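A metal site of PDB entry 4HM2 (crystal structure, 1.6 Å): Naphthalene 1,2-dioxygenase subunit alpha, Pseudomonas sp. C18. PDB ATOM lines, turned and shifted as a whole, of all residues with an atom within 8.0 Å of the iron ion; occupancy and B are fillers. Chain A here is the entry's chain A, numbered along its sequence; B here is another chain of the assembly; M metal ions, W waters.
ND2 of Asn 201 is in hydrogen-bond range of OH of Tyr 103 of chain B. The backbone carbonyl oxygen (O) of Asp 205 lies within hydrogen-bond range of a ring nitrogen (ND1) of His 208, 2.7 Å away. ND2 of Asn 201 sits close to ND1 of His 208. The side-chain amide nitrogen (ND2) of Asn 201 lies within hydrogen-bond range of the side-chain carboxylate (OD2) of Asp 205, 3.4 Å away. The side-chain hydroxyl (OG1) of Thr 212 sits close to the backbone carbonyl oxygen (O) of His 208 (3.5 Å). A ring nitrogen (ND1) of His 213 sits at hydrogen-bond distance from the side-chain carboxylate (OD2) of Asp 361 (2.9 Å). A ring nitrogen (ND1) of His 213 sits close to the backbone carbonyl oxygen (O) of Trp 358, 3.2 Å away.
Asn 201 touches the iron ion. Four residues have an atom within 4 Å of the iron ion: Asn 201, His 208, His 213 and Asp 362. Along chain A the residues within 4 Å of the iron ion span positions 201 to 362. The nearest printed residue that does not touch the iron ion is Thr 212 (4.4 Å).
The iron ion is bound by water W1 (2.0 Å), NE2 of His 213 (2.0 Å), NE2 of His 208 (2.1 Å), OD1 of Asp 362 (2.2 Å) and OD2 of Asp 362 (2.4 Å). The iron ion has five donor atoms within binding distance.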
ATOM      1  N   ASN A 201     -26.588   6.709   1.325  1.00  0.00           N
ATOM      2  CA  ASN A 201     -26.275   7.629   2.405  1.00  0.00           C
ATOM      3  C   ASN A 201     -27.496   8.481   2.733  1.00  0.00           C
ATOM      4  O   ASN A 201     -27.887   8.574   3.891  1.00  0.00           O
ATOM      5  CB  ASN A 201     -25.069   8.489   2.014  1.00  0.00           C
ATOM      6  CG  ASN A 201     -24.706   9.513   3.071  1.00  0.00           C
ATOM      7  OD1 ASN A 201     -25.221  10.632   3.065  1.00  0.00           O
ATOM      8  ND2 ASN A 201     -23.843   9.139   4.003  1.00  0.00           N
ATOM      9  N   PHE A 202     -28.127   9.069   1.714  1.00  0.00           N
ATOM     10  CA  PHE A 202     -29.330   9.871   1.961  1.00  0.00           C
ATOM     11  C   PHE A 202     -30.547   9.062   2.403  1.00  0.00           C
ATOM     12  O   PHE A 202     -31.383   9.591   3.142  1.00  0.00           O
ATOM     13  CB  PHE A 202     -29.674  10.752   0.757  1.00  0.00           C
ATOM     14  CG  PHE A 202     -28.891  12.026   0.692  1.00  0.00           C
ATOM     15  CD1 PHE A 202     -27.510  11.988   0.529  1.00  0.00           C
ATOM     16  CD2 PHE A 202     -29.527  13.253   0.797  1.00  0.00           C
ATOM     17  CE1 PHE A 202     -26.772  13.159   0.468  1.00  0.00           C
ATOM     18  CE2 PHE A 202     -28.792  14.438   0.726  1.00  0.00           C
ATOM     19  CZ  PHE A 202     -27.406  14.387   0.563  1.00  0.00           C
ATOM     20  N   ASP A 205     -28.691   6.952   6.359  1.00  0.00           N
ATOM     21  CA  ASP A 205     -27.449   7.039   7.117  1.00  0.00           C
ATOM     22  C   ASP A 205     -27.390   8.218   8.091  1.00  0.00           C
ATOM     23  O   ASP A 205     -26.751   9.233   7.813  1.00  0.00           O
ATOM     24  CB  ASP A 205     -26.272   7.115   6.151  1.00  0.00           C
ATOM     25  CG  ASP A 205     -24.940   6.845   6.807  1.00  0.00           C
ATOM     26  OD1 ASP A 205     -24.815   6.991   8.047  1.00  0.00           O
ATOM     27  OD2 ASP A 205     -23.990   6.500   6.063  1.00  0.00           O
ATOM     28  N   HIS A 208     -23.558   8.341  10.215  1.00  0.00           N
ATOM     29  CA  HIS A 208     -22.326   9.003   9.768  1.00  0.00           C
ATOM     30  C   HIS A 208     -22.230  10.457  10.180  1.00  0.00           C
ATOM     31  O   HIS A 208     -21.135  11.028  10.200  1.00  0.00           O
ATOM     32  CB  HIS A 208     -22.142   8.872   8.251  1.00  0.00           C
ATOM     33  CG  HIS A 208     -22.821   9.947   7.453  1.00  0.00           C
ATOM     34  ND1 HIS A 208     -24.192  10.031   7.344  1.00  0.00           N
ATOM     35  CD2 HIS A 208     -22.319  10.964   6.722  1.00  0.00           C
ATOM     36  CE1 HIS A 208     -24.503  11.074   6.578  1.00  0.00           C
ATOM     37  NE2 HIS A 208     -23.375  11.649   6.185  1.00  0.00           N
ATOM     38  N   VAL A 209     -23.362  11.078  10.506  1.00  0.00           N
ATOM     39  CA  VAL A 209     -23.411  12.538  10.617  1.00  0.00           C
ATOM     40  C   VAL A 209     -22.445  13.142  11.637  1.00  0.00           C
ATOM     41  O   VAL A 209     -21.675  14.047  11.301  1.00  0.00           O
ATOM     42  CB  VAL A 209     -24.863  13.039  10.851  1.00  0.00           C
ATOM     43  CG1 VAL A 209     -24.883  14.552  11.033  1.00  0.00           C
ATOM     44  CG2 VAL A 209     -25.752  12.621   9.684  1.00  0.00           C
ATOM     45  N   THR A 212     -18.511  11.988  10.228  1.00  0.00           N
ATOM     46  CA  THR A 212     -18.202  12.551   8.902  1.00  0.00           C
ATOM     47  C   THR A 212     -18.277  14.072   8.887  1.00  0.00           C
ATOM     48  O   THR A 212     -17.385  14.760   8.372  1.00  0.00           O
ATOM     49  CB  THR A 212     -19.155  12.018   7.807  1.00  0.00           C
ATOM     50  OG1 THR A 212     -18.905  10.619   7.551  1.00  0.00           O
ATOM     51  CG2 THR A 212     -18.968  12.800   6.506  1.00  0.00           C
ATOM     52  N   HIS A 213     -19.356  14.601   9.466  1.00  0.00           N
ATOM     53  CA  HIS A 213     -19.622  16.034   9.391  1.00  0.00           C
ATOM     54  C   HIS A 213     -19.222  16.783  10.658  1.00  0.00           C
ATOM     55  O   HIS A 213     -19.702  17.896  10.896  1.00  0.00           O
ATOM     56  CB  HIS A 213     -21.098  16.303   9.052  1.00  0.00           C
ATOM     57  CG  HIS A 213     -21.514  15.766   7.712  1.00  0.00           C
ATOM     58  ND1 HIS A 213     -21.102  16.332   6.533  1.00  0.00           N
ATOM     59  CD2 HIS A 213     -22.295  14.715   7.378  1.00  0.00           C
ATOM     60  CE1 HIS A 213     -21.614  15.654   5.522  1.00  0.00           C
ATOM     61  NE2 HIS A 213     -22.349  14.669   6.006  1.00  0.00           N
ATOM     62  N   LEU A 307     -33.290  16.359   1.480  1.00  0.00           N
ATOM     63  CA  LEU A 307     -33.402  16.660   2.900  1.00  0.00           C
ATOM     64  C   LEU A 307     -34.510  17.694   3.007  1.00  0.00           C
ATOM     65  O   LEU A 307     -34.300  18.843   2.616  1.00  0.00           O
ATOM     66  CB  LEU A 307     -32.109  17.271   3.431  1.00  0.00           C
ATOM     67  CG  LEU A 307     -30.809  16.500   3.157  1.00  0.00           C
ATOM     68  CD1 LEU A 307     -29.585  17.245   3.710  1.00  0.00           C
ATOM     69  CD2 LEU A 307     -30.884  15.094   3.750  1.00  0.00           C
ATOM     70  N   PHE A 352     -24.627  22.203   0.700  1.00  0.00           N
ATOM     71  CA  PHE A 352     -24.655  20.960  -0.075  1.00  0.00           C
ATOM     72  C   PHE A 352     -24.466  21.107  -1.576  1.00  0.00           C
ATOM     73  O   PHE A 352     -24.565  20.127  -2.322  1.00  0.00           O
ATOM     74  CB  PHE A 352     -25.958  20.186   0.215  1.00  0.00           C
ATOM     75  CG  PHE A 352     -25.897  19.367   1.469  1.00  0.00           C
ATOM     76  CD1 PHE A 352     -26.238  19.918   2.696  1.00  0.00           C
ATOM     77  CD2 PHE A 352     -25.493  18.039   1.418  1.00  0.00           C
ATOM     78  CE1 PHE A 352     -26.178  19.156   3.860  1.00  0.00           C
ATOM     79  CE2 PHE A 352     -25.445  17.272   2.579  1.00  0.00           C
ATOM     80  CZ  PHE A 352     -25.771  17.829   3.799  1.00  0.00           C
ATOM     81  N   TRP A 358     -20.658  20.975   3.789  1.00  0.00           N
ATOM     82  CA  TRP A 358     -21.141  19.706   4.336  1.00  0.00           C
ATOM     83  C   TRP A 358     -20.909  18.591   3.320  1.00  0.00           C
ATOM     84  O   TRP A 358     -20.339  17.553   3.653  1.00  0.00           O
ATOM     85  CB  TRP A 358     -22.639  19.750   4.698  1.00  0.00           C
ATOM     86  CG  TRP A 358     -22.986  20.612   5.899  1.00  0.00           C
ATOM     87  CD1 TRP A 358     -22.867  21.964   5.992  1.00  0.00           C
ATOM     88  CD2 TRP A 358     -23.555  20.176   7.141  1.00  0.00           C
ATOM     89  NE1 TRP A 358     -23.312  22.404   7.219  1.00  0.00           N
ATOM     90  CE2 TRP A 358     -23.733  21.313   7.944  1.00  0.00           C
ATOM     91  CE3 TRP A 358     -23.916  18.918   7.655  1.00  0.00           C
ATOM     92  CZ2 TRP A 358     -24.264  21.255   9.246  1.00  0.00           C
ATOM     93  CZ3 TRP A 358     -24.444  18.860   8.948  1.00  0.00           C
ATOM     94  CH2 TRP A 358     -24.606  20.017   9.715  1.00  0.00           C
ATOM     95  N   GLU A 359     -21.355  18.811   2.087  1.00  0.00           N
ATOM     96  CA  GLU A 359     -21.252  17.794   1.047  1.00  0.00           C
ATOM     97  C   GLU A 359     -19.800  17.401   0.819  1.00  0.00           C
ATOM     98  O   GLU A 359     -19.491  16.246   0.518  1.00  0.00           O
ATOM     99  CB  GLU A 359     -21.902  18.302  -0.259  1.00  0.00           C
ATOM    100  CG  GLU A 359     -21.776  17.343  -1.456  1.00  0.00           C
ATOM    101  CD  GLU A 359     -23.078  16.672  -1.858  1.00  0.00           C
ATOM    102  OE1 GLU A 359     -23.980  16.513  -0.998  1.00  0.00           O
ATOM    103  OE2 GLU A 359     -23.205  16.290  -3.041  1.00  0.00           O
ATOM    104  N   SER A 360     -18.882  18.356   0.993  1.00  0.00           N
ATOM    105  CA  SER A 360     -17.463  18.058   0.804  1.00  0.00           C
ATOM    106  C   SER A 360     -16.971  17.015   1.817  1.00  0.00           C
ATOM    107  O   SER A 360     -16.074  16.215   1.499  1.00  0.00           O
ATOM    108  CB  SER A 360     -16.610  19.327   0.868  1.00  0.00           C
ATOM    109  OG  SER A 360     -16.412  19.767   2.203  1.00  0.00           O
ATOM    110  N   ASP A 361     -17.550  17.002   3.018  1.00  0.00           N
ATOM    111  CA  ASP A 361     -17.162  16.032   4.042  1.00  0.00           C
ATOM    112  C   ASP A 361     -17.399  14.601   3.558  1.00  0.00           C
ATOM    113  O   ASP A 361     -16.748  13.663   4.028  1.00  0.00           O
ATOM    114  CB  ASP A 361     -17.969  16.227   5.335  1.00  0.00           C
ATOM    115  CG  ASP A 361     -17.806  17.603   5.953  1.00  0.00           C
ATOM    116  OD1 ASP A 361     -16.775  18.276   5.748  1.00  0.00           O
ATOM    117  OD2 ASP A 361     -18.735  18.017   6.685  1.00  0.00           O
ATOM    118  N   ASP A 362     -18.343  14.453   2.630  1.00  0.00           N
ATOM    119  CA  ASP A 362     -18.747  13.115   2.183  1.00  0.00           C
ATOM    120  C   ASP A 362     -17.928  12.570   1.018  1.00  0.00           C
ATOM    121  O   ASP A 362     -18.015  11.377   0.726  1.00  0.00           O
ATOM    122  CB  ASP A 362     -20.221  13.115   1.757  1.00  0.00           C
ATOM    123  CG  ASP A 362     -21.177  13.290   2.922  1.00  0.00           C
ATOM    124  OD1 ASP A 362     -21.267  12.393   3.787  1.00  0.00           O
ATOM    125  OD2 ASP A 362     -21.896  14.303   2.934  1.00  0.00           O
ATOM    126  N   ASN A 363     -17.167  13.444   0.339  1.00  0.00           N
ATOM    127  CA  ASN A 363     -16.494  13.080  -0.923  1.00  0.00           C
ATOM    128  C   ASN A 363     -15.638  11.829  -0.803  1.00  0.00           C
ATOM    129  O   ASN A 363     -15.839  10.869  -1.551  1.00  0.00           O
ATOM    130  CB  ASN A 363     -15.567  14.196  -1.416  1.00  0.00           C
ATOM    131  CG  ASN A 363     -16.311  15.358  -2.039  1.00  0.00           C
ATOM    132  OD1 ASN A 363     -15.705  16.397  -2.323  1.00  0.00           O
ATOM    133  ND2 ASN A 363     -17.619  15.204  -2.250  1.00  0.00           N
ATOM    134  N   ASN A 365     -15.375   9.575   1.519  1.00  0.00           N
ATOM    135  CA  ASN A 365     -16.125   8.407   1.958  1.00  0.00           C
ATOM    136  C   ASN A 365     -16.794   7.719   0.776  1.00  0.00           C
ATOM    137  O   ASN A 365     -16.670   6.501   0.594  1.00  0.00           O
ATOM    138  CB  ASN A 365     -17.191   8.799   2.986  1.00  0.00           C
ATOM    139  CG  ASN A 365     -16.605   9.260   4.310  1.00  0.00           C
ATOM    140  OD1 ASN A 365     -15.482   8.900   4.665  1.00  0.00           O
ATOM    141  ND2 ASN A 365     -17.372  10.054   5.049  1.00  0.00           N
ATOM    142  N   MET A 366     -17.515   8.485  -0.028  1.00  0.00           N
ATOM    143  CA  MET A 366     -18.257   7.878  -1.119  1.00  0.00           C
ATOM    144  C   MET A 366     -17.385   7.477  -2.296  1.00  0.00           C
ATOM    145  O   MET A 366     -17.630   6.442  -2.935  1.00  0.00           O
ATOM    146  CB  MET A 366     -19.394   8.788  -1.550  1.00  0.00           C
ATOM    147  CG  MET A 366     -20.466   8.927  -0.487  1.00  0.00           C
ATOM    148  SD  MET A 366     -21.527  10.278  -0.957  1.00  0.00           S
ATOM    149  CE  MET A 366     -22.534  10.483   0.516  1.00  0.00           C
ATOM    150  N   TYR B 103     -15.805   7.566   8.074  1.00  0.00           N
ATOM    151  CA  TYR B 103     -17.214   7.516   7.660  1.00  0.00           C
ATOM    152  C   TYR B 103     -18.119   7.409   8.903  1.00  0.00           C
ATOM    153  O   TYR B 103     -18.792   8.387   9.253  1.00  0.00           O
ATOM    154  CB  TYR B 103     -17.425   6.380   6.653  1.00  0.00           C
ATOM    155  CG  TYR B 103     -18.664   6.496   5.763  1.00  0.00           C
ATOM    156  CD1 TYR B 103     -19.691   7.395   6.057  1.00  0.00           C
ATOM    157  CD2 TYR B 103     -18.789   5.704   4.631  1.00  0.00           C
ATOM    158  CE1 TYR B 103     -20.813   7.485   5.245  1.00  0.00           C
ATOM    159  CE2 TYR B 103     -19.921   5.789   3.806  1.00  0.00           C
ATOM    160  CZ  TYR B 103     -20.923   6.684   4.126  1.00  0.00           C
ATOM    161  OH  TYR B 103     -22.035   6.770   3.316  1.00  0.00           O
HETATM  162 FE    FE M   1     -23.004  13.206   4.805  1.00  0.00          FE
HETATM  163  O   HOH W   1     -24.516  13.149   3.544  1.00  0.00           O
